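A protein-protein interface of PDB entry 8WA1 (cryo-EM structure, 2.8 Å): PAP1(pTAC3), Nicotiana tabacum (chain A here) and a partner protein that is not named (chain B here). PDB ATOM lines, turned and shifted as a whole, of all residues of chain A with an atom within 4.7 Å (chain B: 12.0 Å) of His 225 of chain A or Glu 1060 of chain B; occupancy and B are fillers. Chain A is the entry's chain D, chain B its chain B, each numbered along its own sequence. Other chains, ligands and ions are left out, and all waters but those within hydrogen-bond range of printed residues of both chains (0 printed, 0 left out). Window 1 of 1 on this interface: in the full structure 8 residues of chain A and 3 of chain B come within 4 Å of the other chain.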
ATOM      1  N   GLY A 223       4.833  14.742 -14.919  1.00  0.00           N
ATOM      2  CA  GLY A 223       5.254  13.355 -14.898  1.00  0.00           C
ATOM      3  C   GLY A 223       5.935  12.918 -16.178  1.00  0.00           C
ATOM      4  O   GLY A 223       6.184  11.727 -16.382  1.00  0.00           O
ATOM      5  N   ASP A 224       6.242  13.878 -17.050  1.00  0.00           N
ATOM      6  CA  ASP A 224       6.872  13.593 -18.339  1.00  0.00           C
ATOM      7  C   ASP A 224       8.380  13.702 -18.159  1.00  0.00           C
ATOM      8  O   ASP A 224       8.964  14.783 -18.240  1.00  0.00           O
ATOM      9  CB  ASP A 224       6.353  14.543 -19.410  1.00  0.00           C
ATOM     10  CG  ASP A 224       6.670  14.072 -20.816  1.00  0.00           C
ATOM     11  OD1 ASP A 224       7.397  13.065 -20.962  1.00  0.00           O
ATOM     12  OD2 ASP A 224       6.187  14.706 -21.775  1.00  0.00           O
ATOM     13  N   HIS A 225       9.023  12.558 -17.909  1.00  0.00           N
ATOM     14  CA  HIS A 225      10.465  12.551 -17.682  1.00  0.00           C
ATOM     15  C   HIS A 225      11.238  12.642 -18.993  1.00  0.00           C
ATOM     16  O   HIS A 225      12.360  13.161 -19.021  1.00  0.00           O
ATOM     17  CB  HIS A 225      10.868  11.297 -16.909  1.00  0.00           C
ATOM     18  CG  HIS A 225      12.343  11.163 -16.696  1.00  0.00           C
ATOM     19  ND1 HIS A 225      13.154  10.436 -17.541  1.00  0.00           N
ATOM     20  CD2 HIS A 225      13.155  11.664 -15.735  1.00  0.00           C
ATOM     21  CE1 HIS A 225      14.401  10.495 -17.109  1.00  0.00           C
ATOM     22  NE2 HIS A 225      14.429  11.233 -16.015  1.00  0.00           N
ATOM     23  N   SER A 226      10.657  12.143 -20.087  1.00  0.00           N
ATOM     24  CA  SER A 226      11.371  12.110 -21.359  1.00  0.00           C
ATOM     25  C   SER A 226      11.657  13.516 -21.871  1.00  0.00           C
ATOM     26  O   SER A 226      12.799  13.845 -22.217  1.00  0.00           O
ATOM     27  CB  SER A 226      10.566  11.315 -22.388  1.00  0.00           C
ATOM     28  OG  SER A 226       9.290  11.894 -22.589  1.00  0.00           O
ATOM     29  N   ASN A 227      10.625  14.361 -21.938  1.00  0.00           N
ATOM     30  CA  ASN A 227      10.824  15.724 -22.416  1.00  0.00           C
ATOM     31  C   ASN A 227      11.710  16.521 -21.467  1.00  0.00           C
ATOM     32  O   ASN A 227      12.501  17.359 -21.909  1.00  0.00           O
ATOM     33  CB  ASN A 227       9.477  16.417 -22.612  1.00  0.00           C
ATOM     34  CG  ASN A 227       8.816  16.040 -23.922  1.00  0.00           C
ATOM     35  OD1 ASN A 227       7.666  15.606 -23.949  1.00  0.00           O
ATOM     36  ND2 ASN A 227       9.546  16.201 -25.018  1.00  0.00           N
ATOM     37  N   ALA A 228      11.598  16.269 -20.160  1.00  0.00           N
ATOM     38  CA  ALA A 228      12.468  16.946 -19.205  1.00  0.00           C
ATOM     39  C   ALA A 228      13.930  16.583 -19.439  1.00  0.00           C
ATOM     40  O   ALA A 228      14.803  17.459 -19.444  1.00  0.00           O
ATOM     41  CB  ALA A 228      12.049  16.601 -17.777  1.00  0.00           C
ATOM     42  N   LEU A 229      14.212  15.295 -19.647  1.00  0.00           N
ATOM     43  CA  LEU A 229      15.584  14.869 -19.903  1.00  0.00           C
ATOM     44  C   LEU A 229      16.089  15.415 -21.233  1.00  0.00           C
ATOM     45  O   LEU A 229      17.265  15.779 -21.358  1.00  0.00           O
ATOM     46  CB  LEU A 229      15.672  13.343 -19.875  1.00  0.00           C
ATOM     47  CG  LEU A 229      17.070  12.730 -19.966  1.00  0.00           C
ATOM     48  CD1 LEU A 229      17.949  13.229 -18.831  1.00  0.00           C
ATOM     49  CD2 LEU A 229      16.991  11.212 -19.960  1.00  0.00           C
ATOM     50  N   LEU A 250      14.237  15.725 -11.786  1.00  0.00           N
ATOM     51  CA  LEU A 250      14.249  14.466 -12.526  1.00  0.00           C
ATOM     52  C   LEU A 250      14.046  13.274 -11.598  1.00  0.00           C
ATOM     53  O   LEU A 250      13.299  12.346 -11.927  1.00  0.00           O
ATOM     54  CB  LEU A 250      15.557  14.324 -13.305  1.00  0.00           C
ATOM     55  CG  LEU A 250      15.517  14.730 -14.780  1.00  0.00           C
ATOM     56  CD1 LEU A 250      15.062  16.171 -14.945  1.00  0.00           C
ATOM     57  CD2 LEU A 250      16.876  14.518 -15.430  1.00  0.00           C
ATOM     58  N   VAL A 253      10.498  12.250 -10.593  1.00  0.00           N
ATOM     59  CA  VAL A 253       9.785  11.338 -11.481  1.00  0.00           C
ATOM     60  C   VAL A 253      10.447   9.965 -11.483  1.00  0.00           C
ATOM     61  O   VAL A 253       9.767   8.932 -11.548  1.00  0.00           O
ATOM     62  CB  VAL A 253       9.708  11.932 -12.900  1.00  0.00           C
ATOM     63  CG1 VAL A 253       8.907  11.020 -13.817  1.00  0.00           C
ATOM     64  CG2 VAL A 253       9.098  13.322 -12.860  1.00  0.00           C
ATOM     65  N   GLN A 254      11.780   9.927 -11.406  1.00  0.00           N
ATOM     66  CA  GLN A 254      12.501   8.659 -11.467  1.00  0.00           C
ATOM     67  C   GLN A 254      12.217   7.759 -10.270  1.00  0.00           C
ATOM     68  O   GLN A 254      12.359   6.537 -10.384  1.00  0.00           O
ATOM     69  CB  GLN A 254      14.008   8.905 -11.563  1.00  0.00           C
ATOM     70  CG  GLN A 254      14.472   9.533 -12.869  1.00  0.00           C
ATOM     71  CD  GLN A 254      15.980   9.697 -12.928  1.00  0.00           C
ATOM     72  OE1 GLN A 254      16.709   9.142 -12.105  1.00  0.00           O
ATOM     73  NE2 GLN A 254      16.455  10.463 -13.903  1.00  0.00           N
ATOM     74  N   HIS B1055      17.255 -10.222 -22.497  1.00  0.00           N
ATOM     75  CA  HIS B1055      18.039  -8.992 -22.523  1.00  0.00           C
ATOM     76  C   HIS B1055      17.407  -7.921 -21.640  1.00  0.00           C
ATOM     77  O   HIS B1055      18.052  -7.407 -20.719  1.00  0.00           O
ATOM     78  CB  HIS B1055      18.183  -8.495 -23.961  1.00  0.00           C
ATOM     79  CG  HIS B1055      19.130  -7.346 -24.116  1.00  0.00           C
ATOM     80  ND1 HIS B1055      19.867  -6.840 -23.067  1.00  0.00           N
ATOM     81  CD2 HIS B1055      19.460  -6.606 -25.200  1.00  0.00           C
ATOM     82  CE1 HIS B1055      20.607  -5.834 -23.498  1.00  0.00           C
ATOM     83  NE2 HIS B1055      20.380  -5.672 -24.790  1.00  0.00           N
ATOM     84  N   PHE B1056      16.150  -7.569 -21.912  1.00  0.00           N
ATOM     85  CA  PHE B1056      15.376  -6.648 -21.082  1.00  0.00           C
ATOM     86  C   PHE B1056      16.084  -5.304 -20.909  1.00  0.00           C
ATOM     87  O   PHE B1056      16.537  -4.943 -19.823  1.00  0.00           O
ATOM     88  CB  PHE B1056      15.062  -7.273 -19.722  1.00  0.00           C
ATOM     89  CG  PHE B1056      13.866  -8.174 -19.725  1.00  0.00           C
ATOM     90  CD1 PHE B1056      12.838  -7.982 -20.634  1.00  0.00           C
ATOM     91  CD2 PHE B1056      13.764  -9.211 -18.816  1.00  0.00           C
ATOM     92  CE1 PHE B1056      11.734  -8.811 -20.634  1.00  0.00           C
ATOM     93  CE2 PHE B1056      12.665 -10.043 -18.813  1.00  0.00           C
ATOM     94  CZ  PHE B1056      11.648  -9.844 -19.723  1.00  0.00           C
ATOM     95  N   LEU B1057      16.190  -4.568 -22.011  1.00  0.00           N
ATOM     96  CA  LEU B1057      16.713  -3.211 -21.940  1.00  0.00           C
ATOM     97  C   LEU B1057      15.604  -2.242 -21.547  1.00  0.00           C
ATOM     98  O   LEU B1057      14.454  -2.389 -21.971  1.00  0.00           O
ATOM     99  CB  LEU B1057      17.339  -2.810 -23.275  1.00  0.00           C
ATOM    100  CG  LEU B1057      16.727  -3.375 -24.556  1.00  0.00           C
ATOM    101  CD1 LEU B1057      15.488  -2.605 -24.969  1.00  0.00           C
ATOM    102  CD2 LEU B1057      17.753  -3.359 -25.668  1.00  0.00           C
ATOM    103  N   VAL B1058      15.949  -1.256 -20.723  1.00  0.00           N
ATOM    104  CA  VAL B1058      14.993  -0.299 -20.177  1.00  0.00           C
ATOM    105  C   VAL B1058      15.309   1.075 -20.750  1.00  0.00           C
ATOM    106  O   VAL B1058      16.467   1.506 -20.739  1.00  0.00           O
ATOM    107  CB  VAL B1058      15.040  -0.277 -18.639  1.00  0.00           C
ATOM    108  CG1 VAL B1058      13.981   0.661 -18.083  1.00  0.00           C
ATOM    109  CG2 VAL B1058      14.869  -1.682 -18.084  1.00  0.00           C
ATOM    110  N   SER B1059      14.283   1.760 -21.248  1.00  0.00           N
ATOM    111  CA  SER B1059      14.472   3.094 -21.797  1.00  0.00           C
ATOM    112  C   SER B1059      14.514   4.128 -20.679  1.00  0.00           C
ATOM    113  O   SER B1059      13.649   4.151 -19.801  1.00  0.00           O
ATOM    114  CB  SER B1059      13.355   3.433 -22.784  1.00  0.00           C
ATOM    115  OG  SER B1059      12.087   3.410 -22.154  1.00  0.00           O
ATOM    116  N   GLU B1060      15.536   4.987 -20.720  1.00  0.00           N
ATOM    117  CA  GLU B1060      15.682   6.013 -19.692  1.00  0.00           C
ATOM    118  C   GLU B1060      14.652   7.122 -19.867  1.00  0.00           C
ATOM    119  O   GLU B1060      14.361   7.865 -18.923  1.00  0.00           O
ATOM    120  CB  GLU B1060      17.101   6.588 -19.716  1.00  0.00           C
ATOM    121  CG  GLU B1060      17.412   7.475 -20.917  1.00  0.00           C
ATOM    122  CD  GLU B1060      17.605   6.690 -22.200  1.00  0.00           C
ATOM    123  OE1 GLU B1060      17.762   5.453 -22.126  1.00  0.00           O
ATOM    124  OE2 GLU B1060      17.599   7.310 -23.283  1.00  0.00           O
ATOM    125  N   LYS B1061      14.093   7.253 -21.072  1.00  0.00           N
ATOM    126  CA  LYS B1061      13.144   8.330 -21.338  1.00  0.00           C
ATOM    127  C   LYS B1061      11.809   8.082 -20.642  1.00  0.00           C
ATOM    128  O   LYS B1061      11.342   8.918 -19.859  1.00  0.00           O
ATOM    129  CB  LYS B1061      12.941   8.485 -22.846  1.00  0.00           C
ATOM    130  CG  LYS B1061      14.197   8.866 -23.607  1.00  0.00           C
ATOM    131  CD  LYS B1061      14.718  10.224 -23.167  1.00  0.00           C
ATOM    132  CE  LYS B1061      15.958  10.622 -23.948  1.00  0.00           C
ATOM    133  NZ  LYS B1061      16.466  11.963 -23.546  1.00  0.00           N
ATOM    134  N   ASN B1062      11.184   6.935 -20.910  1.00  0.00           N
ATOM    135  CA  ASN B1062       9.829   6.663 -20.444  1.00  0.00           C
ATOM    136  C   ASN B1062       9.750   5.491 -19.471  1.00  0.00           C
ATOM    137  O   ASN B1062       8.640   5.082 -19.111  1.00  0.00           O
ATOM    138  CB  ASN B1062       8.906   6.412 -21.640  1.00  0.00           C
ATOM    139  CG  ASN B1062       9.616   5.724 -22.788  1.00  0.00           C
ATOM    140  OD1 ASN B1062      10.034   6.368 -23.749  1.00  0.00           O
ATOM    141  ND2 ASN B1062       9.763   4.409 -22.690  1.00  0.00           N
ATOM    142  N   PHE B1063      10.888   4.945 -19.044  1.00  0.00           N
ATOM    143  CA  PHE B1063      10.936   3.907 -18.012  1.00  0.00           C
ATOM    144  C   PHE B1063      10.115   2.681 -18.412  1.00  0.00           C
ATOM    145  O   PHE B1063       9.261   2.200 -17.664  1.00  0.00           O
ATOM    146  CB  PHE B1063      10.471   4.458 -16.663  1.00  0.00           C
ATOM    147  CG  PHE B1063      11.216   5.685 -16.219  1.00  0.00           C
ATOM    148  CD1 PHE B1063      12.565   5.833 -16.500  1.00  0.00           C
ATOM    149  CD2 PHE B1063      10.567   6.692 -15.525  1.00  0.00           C
ATOM    150  CE1 PHE B1063      13.250   6.960 -16.095  1.00  0.00           C
ATOM    151  CE2 PHE B1063      11.248   7.822 -15.118  1.00  0.00           C
ATOM    152  CZ  PHE B1063      12.591   7.956 -15.403  1.00  0.00           C
ATOM    153  N   GLN B1064      10.380   2.173 -19.613  1.00  0.00           N
ATOM    154  CA  GLN B1064       9.695   1.003 -20.139  1.00  0.00           C
ATOM    155  C   GLN B1064      10.699  -0.107 -20.414  1.00  0.00           C
ATOM    156  O   GLN B1064      11.812   0.150 -20.882  1.00  0.00           O
ATOM    157  CB  GLN B1064       8.925   1.338 -21.417  1.00  0.00           C
ATOM    158  CG  GLN B1064       7.754   2.282 -21.203  1.00  0.00           C
ATOM    159  CD  GLN B1064       7.037   2.616 -22.494  1.00  0.00           C
ATOM    160  OE1 GLN B1064       6.085   3.395 -22.505  1.00  0.00           O
ATOM    161  NE2 GLN B1064       7.492   2.026 -23.593  1.00  0.00           N
ATOM    162  N   ILE B1065      10.296  -1.342 -20.121  1.00  0.00           N
ATOM    163  CA  ILE B1065      11.129  -2.520 -20.330  1.00  0.00           C
ATOM    164  C   ILE B1065      10.779  -3.126 -21.682  1.00  0.00           C
ATOM    165  O   ILE B1065       9.602  -3.377 -21.972  1.00  0.00           O
ATOM    166  CB  ILE B1065      10.935  -3.546 -19.201  1.00  0.00           C
ATOM    167  CG1 ILE B1065      11.207  -2.901 -17.841  1.00  0.00           C
ATOM    168  CG2 ILE B1065      11.840  -4.749 -19.411  1.00  0.00           C
ATOM    169  CD1 ILE B1065      10.990  -3.835 -16.669  1.00  0.00           C
ATOM    170  N   ASN B1066      11.794  -3.359 -22.509  1.00  0.00           N
ATOM    171  CA  ASN B1066      11.613  -3.928 -23.839  1.00  0.00           C
ATOM    172  C   ASN B1066      12.501  -5.156 -23.974  1.00  0.00           C
ATOM    173  O   ASN B1066      13.721  -5.066 -23.806  1.00  0.00           O
ATOM    174  CB  ASN B1066      11.939  -2.901 -24.925  1.00  0.00           C
ATOM    175  CG  ASN B1066      11.149  -1.617 -24.768  1.00  0.00           C
ATOM    176  OD1 ASN B1066       9.991  -1.634 -24.351  1.00  0.00           O
ATOM    177  ND2 ASN B1066      11.774  -0.493 -25.100  1.00  0.00           N
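The side-chain carboxylate (OD1) of Asp 224 of chain A is in hydrogen-bond range of the side-chain hydroxyl (OG) of Ser 226 of chain A, at 2.8 Å.
A ring nitrogen (NE2) of His 225 of chain A lies within hydrogen-bond range of the side-chain amide nitrogen (NE2) of Gln 254 of chain A, 3.0 Å away.
Among the printed residues, pairs that only touch across the chains: His 225 of chain A with Phe 1063 of chain B, Leu 229 of chain A with Glu 1060 of chain B, Leu 229 of chain A with Lys 1061 of chain B and Gln 254 of chain A with Phe 1063 of chain B.
Of the 10 printed residues of chain A, 4 touch a printed residue of chain B.
Among the printed residues, no Asp or Glu carboxylate lies within 4 Å of a Lys or Arg side-chain nitrogen of the other chain.
A ring nitrogen (ND1) of His 225 of chain A lies within hydrogen-bond range of the backbone carbonyl oxygen (O) of Glu 1060 of chain B, at 3.2 Å.
The backbone carbonyl oxygen (O) of Lys 1061 of chain B lies within hydrogen-bond range of a ring nitrogen (ND1) of His 225 of chain A, 3.3 Å away.
N of Ser 226 of chain A lies within hydrogen-bond range of O of Lys 1061 of chain B (3.3 Å).
Of chain B, only Glu 1060, Lys 1061 and Phe 1063 come within 4 Å of His 225 of chain A.
Glu 1060 of chain B touches just these residues of chain A: His 225 (3.2 Å) and Leu 229 (3.9 Å).
No residue of chain B comes within 4 Å of Gly 223 of chain A.
No residue of chain B comes within 4 Å of Asp 224 of chain A.
Ser 226 of chain A touches just one residue of chain B: Lys 1061 (3.3 Å).
No residue of chain B comes within 4 Å of Asn 227 of chain A.
No residue of chain B comes within 4 Å of Ala 228 of chain A.
Leu 229 of chain A touches just these residues of chain B: Glu 1060 (3.9 Å) and Lys 1061 (3.7 Å).
No residue of chain B comes within 4 Å of Val 253 of chain A.
Gln 254 of chain A touches just one residue of chain B: Phe 1063 (3.5 Å).
Of the printed residues of chain A, Phe 1063 of chain B touches His 225 and Gln 254.
Printed residues of chain A within 4 Å of Lys 1061 of chain B: His 225 (3.3 Å), Ser 226 (3.3 Å) and Leu 229 (3.7 Å).
Ser 1059 of chain B touches none of the printed residues of chain A.
Asn 1062 of chain B touches none of the printed residues of chain A.
The nearest residue of chain B that does not touch His 225 of chain A is Asn 1062 of chain B (5.2 Å).
The nearest printed residue of chain A that does not touch Phe 1063 of chain B is Val 253 of chain A (4.02 Å).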
